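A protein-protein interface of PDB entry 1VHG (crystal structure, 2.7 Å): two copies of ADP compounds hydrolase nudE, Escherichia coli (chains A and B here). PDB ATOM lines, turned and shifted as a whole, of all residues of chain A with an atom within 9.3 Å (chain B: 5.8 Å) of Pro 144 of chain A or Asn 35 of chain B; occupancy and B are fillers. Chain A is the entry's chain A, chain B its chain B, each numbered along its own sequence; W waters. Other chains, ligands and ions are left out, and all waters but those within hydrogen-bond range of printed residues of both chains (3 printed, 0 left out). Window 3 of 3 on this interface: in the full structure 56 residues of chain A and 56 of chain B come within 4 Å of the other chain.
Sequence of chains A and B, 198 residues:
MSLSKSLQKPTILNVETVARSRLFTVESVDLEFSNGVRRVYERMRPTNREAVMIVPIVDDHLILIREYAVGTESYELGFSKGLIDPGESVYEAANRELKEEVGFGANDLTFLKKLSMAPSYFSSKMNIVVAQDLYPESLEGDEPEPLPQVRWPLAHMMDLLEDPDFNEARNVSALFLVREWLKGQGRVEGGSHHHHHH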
ATOM      1  N   GLU A  67      33.966  14.039  -6.734  1.00  0.00           N
ATOM      2  CA  GLU A  67      32.871  13.208  -7.237  1.00  0.00           C
ATOM      3  C   GLU A  67      31.600  13.285  -6.417  1.00  0.00           C
ATOM      4  O   GLU A  67      31.571  13.165  -5.203  1.00  0.00           O
ATOM      5  CB  GLU A  67      33.418  11.756  -7.261  1.00  0.00           C
ATOM      6  CG  GLU A  67      32.492  10.740  -7.886  1.00  0.00           C
ATOM      7  CD  GLU A  67      33.207   9.412  -8.083  1.00  0.00           C
ATOM      8  OE1 GLU A  67      32.813   8.610  -8.940  1.00  0.00           O
ATOM      9  OE2 GLU A  67      34.207   9.180  -7.362  1.00  0.00           O
ATOM     10  N   TYR A  68      30.473  13.379  -7.126  1.00  0.00           N
ATOM     11  CA  TYR A  68      29.176  13.436  -6.484  1.00  0.00           C
ATOM     12  C   TYR A  68      28.795  12.140  -5.767  1.00  0.00           C
ATOM     13  O   TYR A  68      28.889  11.061  -6.344  1.00  0.00           O
ATOM     14  CB  TYR A  68      28.103  13.777  -7.522  1.00  0.00           C
ATOM     15  CG  TYR A  68      26.746  13.917  -6.868  1.00  0.00           C
ATOM     16  CD1 TYR A  68      25.792  12.919  -7.021  1.00  0.00           C
ATOM     17  CD2 TYR A  68      26.454  15.037  -6.083  1.00  0.00           C
ATOM     18  CE1 TYR A  68      24.552  13.062  -6.439  1.00  0.00           C
ATOM     19  CE2 TYR A  68      25.204  15.186  -5.512  1.00  0.00           C
ATOM     20  CZ  TYR A  68      24.271  14.196  -5.693  1.00  0.00           C
ATOM     21  OH  TYR A  68      23.040  14.287  -5.096  1.00  0.00           O
ATOM     22  N   ALA A  69      28.307  12.227  -4.566  1.00  0.00           N
ATOM     23  CA  ALA A  69      27.871  11.127  -3.723  1.00  0.00           C
ATOM     24  C   ALA A  69      26.393  11.325  -3.408  1.00  0.00           C
ATOM     25  O   ALA A  69      26.013  12.312  -2.750  1.00  0.00           O
ATOM     26  CB  ALA A  69      28.675  11.147  -2.421  1.00  0.00           C
ATOM     27  N   TYR A  75      29.562  16.726  -3.093  1.00  0.00           N
ATOM     28  CA  TYR A  75      30.772  16.365  -3.791  1.00  0.00           C
ATOM     29  C   TYR A  75      31.857  15.977  -2.822  1.00  0.00           C
ATOM     30  O   TYR A  75      32.267  16.801  -1.999  1.00  0.00           O
ATOM     31  CB  TYR A  75      31.263  17.542  -4.669  1.00  0.00           C
ATOM     32  CG  TYR A  75      30.489  17.544  -5.977  1.00  0.00           C
ATOM     33  CD1 TYR A  75      29.362  18.337  -6.142  1.00  0.00           C
ATOM     34  CD2 TYR A  75      30.890  16.734  -7.026  1.00  0.00           C
ATOM     35  CE1 TYR A  75      28.659  18.319  -7.329  1.00  0.00           C
ATOM     36  CE2 TYR A  75      30.199  16.719  -8.225  1.00  0.00           C
ATOM     37  CZ  TYR A  75      29.075  17.508  -8.367  1.00  0.00           C
ATOM     38  OH  TYR A  75      28.361  17.473  -9.540  1.00  0.00           O
ATOM     39  N   GLU A 101      38.817   7.218 -15.532  1.00  0.00           N
ATOM     40  CA  GLU A 101      38.415   8.347 -14.713  1.00  0.00           C
ATOM     41  C   GLU A 101      39.267   9.587 -14.778  1.00  0.00           C
ATOM     42  O   GLU A 101      38.752  10.684 -14.544  1.00  0.00           O
ATOM     43  CB  GLU A 101      38.309   7.895 -13.245  1.00  0.00           C
ATOM     44  CG  GLU A 101      37.088   7.061 -12.901  1.00  0.00           C
ATOM     45  CD  GLU A 101      36.882   6.975 -11.393  1.00  0.00           C
ATOM     46  OE1 GLU A 101      36.834   8.044 -10.749  1.00  0.00           O
ATOM     47  OE2 GLU A 101      36.810   5.849 -10.831  1.00  0.00           O
ATOM     48  N   GLU A 140      36.850   4.895 -21.859  1.00  0.00           N
ATOM     49  CA  GLU A 140      35.479   5.275 -21.577  1.00  0.00           C
ATOM     50  C   GLU A 140      34.921   4.643 -20.315  1.00  0.00           C
ATOM     51  O   GLU A 140      34.815   3.419 -20.193  1.00  0.00           O
ATOM     52  CB  GLU A 140      34.613   4.882 -22.789  1.00  0.00           C
ATOM     53  CG  GLU A 140      33.950   6.093 -23.439  1.00  0.00           C
ATOM     54  CD  GLU A 140      32.581   6.384 -22.836  1.00  0.00           C
ATOM     55  OE1 GLU A 140      31.988   7.444 -23.140  1.00  0.00           O
ATOM     56  OE2 GLU A 140      32.067   5.552 -22.052  1.00  0.00           O
ATOM     57  N   GLY A 141      34.536   5.471 -19.349  1.00  0.00           N
ATOM     58  CA  GLY A 141      33.981   4.914 -18.095  1.00  0.00           C
ATOM     59  C   GLY A 141      32.464   5.111 -18.089  1.00  0.00           C
ATOM     60  O   GLY A 141      31.868   5.437 -19.117  1.00  0.00           O
ATOM     61  N   ASP A 142      31.848   4.924 -16.933  1.00  0.00           N
ATOM     62  CA  ASP A 142      30.401   5.085 -16.824  1.00  0.00           C
ATOM     63  C   ASP A 142      29.999   6.323 -16.055  1.00  0.00           C
ATOM     64  O   ASP A 142      28.851   6.452 -15.646  1.00  0.00           O
ATOM     65  CB  ASP A 142      29.817   3.816 -16.172  1.00  0.00           C
ATOM     66  CG  ASP A 142      30.237   2.558 -16.927  1.00  0.00           C
ATOM     67  OD1 ASP A 142      29.657   2.287 -18.007  1.00  0.00           O
ATOM     68  OD2 ASP A 142      31.171   1.849 -16.485  1.00  0.00           O
ATOM     69  N   GLU A 143      30.910   7.264 -15.819  1.00  0.00           N
ATOM     70  CA  GLU A 143      30.573   8.468 -15.080  1.00  0.00           C
ATOM     71  C   GLU A 143      29.630   9.357 -15.879  1.00  0.00           C
ATOM     72  O   GLU A 143      29.857   9.600 -17.061  1.00  0.00           O
ATOM     73  CB  GLU A 143      31.825   9.240 -14.683  1.00  0.00           C
ATOM     74  CG  GLU A 143      32.629   9.890 -15.782  1.00  0.00           C
ATOM     75  CD  GLU A 143      33.623   8.969 -16.455  1.00  0.00           C
ATOM     76  OE1 GLU A 143      33.873   9.164 -17.668  1.00  0.00           O
ATOM     77  OE2 GLU A 143      34.173   8.057 -15.785  1.00  0.00           O
ATOM     78  N   PRO A 144      28.648   9.948 -15.220  1.00  0.00           N
ATOM     79  CA  PRO A 144      27.684  10.814 -15.872  1.00  0.00           C
ATOM     80  C   PRO A 144      28.219  12.203 -16.129  1.00  0.00           C
ATOM     81  O   PRO A 144      27.638  12.979 -16.884  1.00  0.00           O
ATOM     82  CB  PRO A 144      26.527  10.876 -14.881  1.00  0.00           C
ATOM     83  CG  PRO A 144      27.149  10.632 -13.560  1.00  0.00           C
ATOM     84  CD  PRO A 144      28.324   9.731 -13.789  1.00  0.00           C
ATOM     85  N   GLU A 145      29.249  12.586 -15.402  1.00  0.00           N
ATOM     86  CA  GLU A 145      29.841  13.927 -15.558  1.00  0.00           C
ATOM     87  C   GLU A 145      31.332  13.746 -15.313  1.00  0.00           C
ATOM     88  O   GLU A 145      31.712  12.777 -14.654  1.00  0.00           O
ATOM     89  CB  GLU A 145      29.218  14.960 -14.652  1.00  0.00           C
ATOM     90  CG  GLU A 145      29.481  14.866 -13.185  1.00  0.00           C
ATOM     91  CD  GLU A 145      28.751  15.824 -12.271  1.00  0.00           C
ATOM     92  OE1 GLU A 145      28.147  16.848 -12.681  1.00  0.00           O
ATOM     93  OE2 GLU A 145      28.801  15.542 -11.030  1.00  0.00           O
ATOM     94  N   PRO A 146      32.129  14.572 -15.945  1.00  0.00           N
ATOM     95  CA  PRO A 146      33.589  14.488 -15.802  1.00  0.00           C
ATOM     96  C   PRO A 146      34.029  14.750 -14.379  1.00  0.00           C
ATOM     97  O   PRO A 146      33.369  15.478 -13.623  1.00  0.00           O
ATOM     98  CB  PRO A 146      34.090  15.563 -16.764  1.00  0.00           C
ATOM     99  CG  PRO A 146      32.976  16.581 -16.757  1.00  0.00           C
ATOM    100  CD  PRO A 146      31.717  15.733 -16.765  1.00  0.00           C
ATOM    101  N   LEU A 147      35.127  14.165 -13.940  1.00  0.00           N
ATOM    102  CA  LEU A 147      35.599  14.372 -12.574  1.00  0.00           C
ATOM    103  C   LEU A 147      36.734  15.359 -12.480  1.00  0.00           C
ATOM    104  O   LEU A 147      37.875  15.122 -12.881  1.00  0.00           O
ATOM    105  CB  LEU A 147      35.963  12.989 -12.014  1.00  0.00           C
ATOM    106  CG  LEU A 147      34.871  11.933 -12.291  1.00  0.00           C
ATOM    107  CD1 LEU A 147      35.470  10.543 -12.186  1.00  0.00           C
ATOM    108  CD2 LEU A 147      33.661  12.115 -11.390  1.00  0.00           C
ATOM    109  N   PHE B  33      22.140  15.623 -13.719  1.00  0.00           N
ATOM    110  CA  PHE B  33      23.404  16.345 -13.527  1.00  0.00           C
ATOM    111  C   PHE B  33      23.364  17.648 -14.312  1.00  0.00           C
ATOM    112  O   PHE B  33      22.607  17.811 -15.265  1.00  0.00           O
ATOM    113  CB  PHE B  33      24.556  15.423 -13.927  1.00  0.00           C
ATOM    114  CG  PHE B  33      24.693  14.231 -13.024  1.00  0.00           C
ATOM    115  CD1 PHE B  33      23.955  13.085 -13.242  1.00  0.00           C
ATOM    116  CD2 PHE B  33      25.567  14.264 -11.941  1.00  0.00           C
ATOM    117  CE1 PHE B  33      24.070  11.985 -12.409  1.00  0.00           C
ATOM    118  CE2 PHE B  33      25.684  13.167 -11.113  1.00  0.00           C
ATOM    119  CZ  PHE B  33      24.941  12.026 -11.341  1.00  0.00           C
ATOM    120  N   SER B  34      24.256  18.576 -14.001  1.00  0.00           N
ATOM    121  CA  SER B  34      24.310  19.860 -14.651  1.00  0.00           C
ATOM    122  C   SER B  34      24.607  19.799 -16.136  1.00  0.00           C
ATOM    123  O   SER B  34      24.252  20.754 -16.855  1.00  0.00           O
ATOM    124  CB  SER B  34      25.327  20.758 -13.943  1.00  0.00           C
ATOM    125  OG  SER B  34      26.578  20.603 -14.565  1.00  0.00           O
ATOM    126  N   ASN B  35      25.164  18.719 -16.667  1.00  0.00           N
ATOM    127  CA  ASN B  35      25.445  18.641 -18.093  1.00  0.00           C
ATOM    128  C   ASN B  35      24.258  18.066 -18.843  1.00  0.00           C
ATOM    129  O   ASN B  35      24.373  17.710 -20.021  1.00  0.00           O
ATOM    130  CB  ASN B  35      26.670  17.768 -18.348  1.00  0.00           C
ATOM    131  CG  ASN B  35      26.442  16.361 -17.826  1.00  0.00           C
ATOM    132  OD1 ASN B  35      25.353  16.049 -17.304  1.00  0.00           O
ATOM    133  ND2 ASN B  35      27.466  15.527 -17.967  1.00  0.00           N
ATOM    134  N   GLY B  36      23.152  17.859 -18.140  1.00  0.00           N
ATOM    135  CA  GLY B  36      21.963  17.295 -18.744  1.00  0.00           C
ATOM    136  C   GLY B  36      21.846  15.788 -18.678  1.00  0.00           C
ATOM    137  O   GLY B  36      20.763  15.309 -19.052  1.00  0.00           O
ATOM    138  N   VAL B  37      22.875  15.039 -18.270  1.00  0.00           N
ATOM    139  CA  VAL B  37      22.744  13.578 -18.186  1.00  0.00           C
ATOM    140  C   VAL B  37      21.783  13.154 -17.085  1.00  0.00           C
ATOM    141  O   VAL B  37      21.774  13.705 -15.976  1.00  0.00           O
ATOM    142  CB  VAL B  37      24.100  12.897 -17.958  1.00  0.00           C
ATOM    143  CG1 VAL B  37      23.941  11.417 -17.628  1.00  0.00           C
ATOM    144  CG2 VAL B  37      25.018  13.057 -19.165  1.00  0.00           C
ATOM    145  N   ARG B  39      20.182  10.061 -14.583  1.00  0.00           N
ATOM    146  CA  ARG B  39      20.568   8.758 -14.055  1.00  0.00           C
ATOM    147  C   ARG B  39      19.816   8.387 -12.796  1.00  0.00           C
ATOM    148  O   ARG B  39      19.290   9.254 -12.094  1.00  0.00           O
ATOM    149  CB  ARG B  39      22.063   8.908 -13.727  1.00  0.00           C
ATOM    150  CG  ARG B  39      22.939   7.803 -14.218  1.00  0.00           C
ATOM    151  CD  ARG B  39      23.277   7.940 -15.713  1.00  0.00           C
ATOM    152  NE  ARG B  39      24.685   7.644 -15.857  1.00  0.00           N
ATOM    153  CZ  ARG B  39      25.510   7.603 -16.864  1.00  0.00           C
ATOM    154  NH1 ARG B  39      25.189   7.849 -18.131  1.00  0.00           N
ATOM    155  NH2 ARG B  39      26.761   7.317 -16.550  1.00  0.00           N
ATOM    156  N   TYR B  41      20.137   6.520  -9.141  1.00  0.00           N
ATOM    157  CA  TYR B  41      21.044   5.967  -8.137  1.00  0.00           C
ATOM    158  C   TYR B  41      20.262   5.266  -7.038  1.00  0.00           C
ATOM    159  O   TYR B  41      19.075   5.457  -6.862  1.00  0.00           O
ATOM    160  CB  TYR B  41      21.948   7.047  -7.551  1.00  0.00           C
ATOM    161  CG  TYR B  41      23.127   7.476  -8.393  1.00  0.00           C
ATOM    162  CD1 TYR B  41      23.151   7.290  -9.763  1.00  0.00           C
ATOM    163  CD2 TYR B  41      24.234   8.093  -7.825  1.00  0.00           C
ATOM    164  CE1 TYR B  41      24.221   7.655 -10.546  1.00  0.00           C
ATOM    165  CE2 TYR B  41      25.312   8.491  -8.596  1.00  0.00           C
ATOM    166  CZ  TYR B  41      25.301   8.266  -9.960  1.00  0.00           C
ATOM    167  OH  TYR B  41      26.361   8.650 -10.740  1.00  0.00           O
HETATM  168  O   HOH W   1      28.014   9.938  -9.352  1.00  0.00           O
HETATM  169  O   HOH W   2      27.416  18.170 -15.140  1.00  0.00           O
HETATM  170  O   HOH W   3      25.891  18.025 -11.813  1.00  0.00           O
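The side-chain carboxylate of Glu 145 of chain A is in hydrogen-bond range of the side-chain hydroxyl of Tyr 75 of chain A, at 2.5 Å. The backbone NH (N) of Val 37 of chain B sits at hydrogen-bond distance from the side-chain amide oxygen (OD1) of Asn 35 of chain B (2.8 Å).
Among the printed residues, merely in contact across the chains: Pro 144 of chain A with Phe 33 of chain B, Pro 144 of chain A with Val 37 of chain B, Pro 144 of chain A with Arg 39 of chain B, Pro 144 of chain A with Tyr 41 of chain B, Glu 145 of chain A with Phe 33 of chain B, Glu 143 of chain A with Arg 39 of chain B and Glu 145 of chain A with Asn 35 of chain B.
Water W1 lies within hydrogen-bond range of OH of Tyr 41 of chain B and O of Tyr 68 of chain A. Water W2 lies within hydrogen-bond range of the side-chain hydroxyl of Ser 34 of chain B, the backbone NH of Asn 35 of chain B and the side-chain carboxylate of Glu 145 of chain A. Water W3 lies within hydrogen-bond range of the side-chain carboxylate (OE1) of Glu 145 of chain A (2.7 Å), the backbone NH (N) of Ser 34 of chain B (2.8 Å) and the side-chain hydroxyl (OH) of Tyr 75 of chain A (3.4 Å).
No position is printed for both chains.
The guanidinium group (NH2) of Arg 39 of chain B lies within hydrogen-bond range of the backbone carbonyl oxygen (O) of Asp 142 of chain A. O of Pro 144 of chain A sits at hydrogen-bond distance from ND2 of Asn 35 of chain B (2.8 Å).
Hydrophobic or aromatic side chains of chain B that line the printed part of chain A: Phe 33, Val 37 and Tyr 41. Along chain B the printed residues that touch a printed residue of chain A span positions 33 to 41. Of the 13 printed residues of chain A, 4 touch a printed residue of chain B. Among the printed residues, 9 pairs touch across the chains. Among the printed residues, no Asp or Glu carboxylate lies within 4 Å of a Lys or Arg side-chain nitrogen of the other chain.
Of chain B, only Phe 33 (3.4 Å), Asn 35 (2.8 Å), Val 37 (3.5 Å), Arg 39 (3.5 Å) and Tyr 41 (3.5 Å) come within 4 Å of Pro 144 of chain A. Printed residues of chain A within 4 Å of Asn 35 of chain B: Pro 144 (2.8 Å) and Glu 145 (3.7 Å). Of chain A, only Pro 144 (3.4 Å) and Glu 145 (3.6 Å) come within 4 Å of Phe 33 of chain B. Ser 34 of chain B touches none of the printed residues of chain A. Printed residues of chain A within 4 Å of Tyr 41 of chain B: Pro 144. Printed residues of chain B within 4 Å of Glu 143 of chain A: Arg 39 (3.6 Å). Pro 146 of chain A touches none of the printed residues of chain B. The nearest printed residue of chain B that does not touch Pro 144 of chain A is Gly 36 of chain B (6.7 Å). The nearest residue of chain A that does not touch Asn 35 of chain B is Pro 146 of chain A (4.4 Å). The nearest printed residue of chain B that does not touch Glu 145 of chain A is Ser 34 of chain B (4.5 Å).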
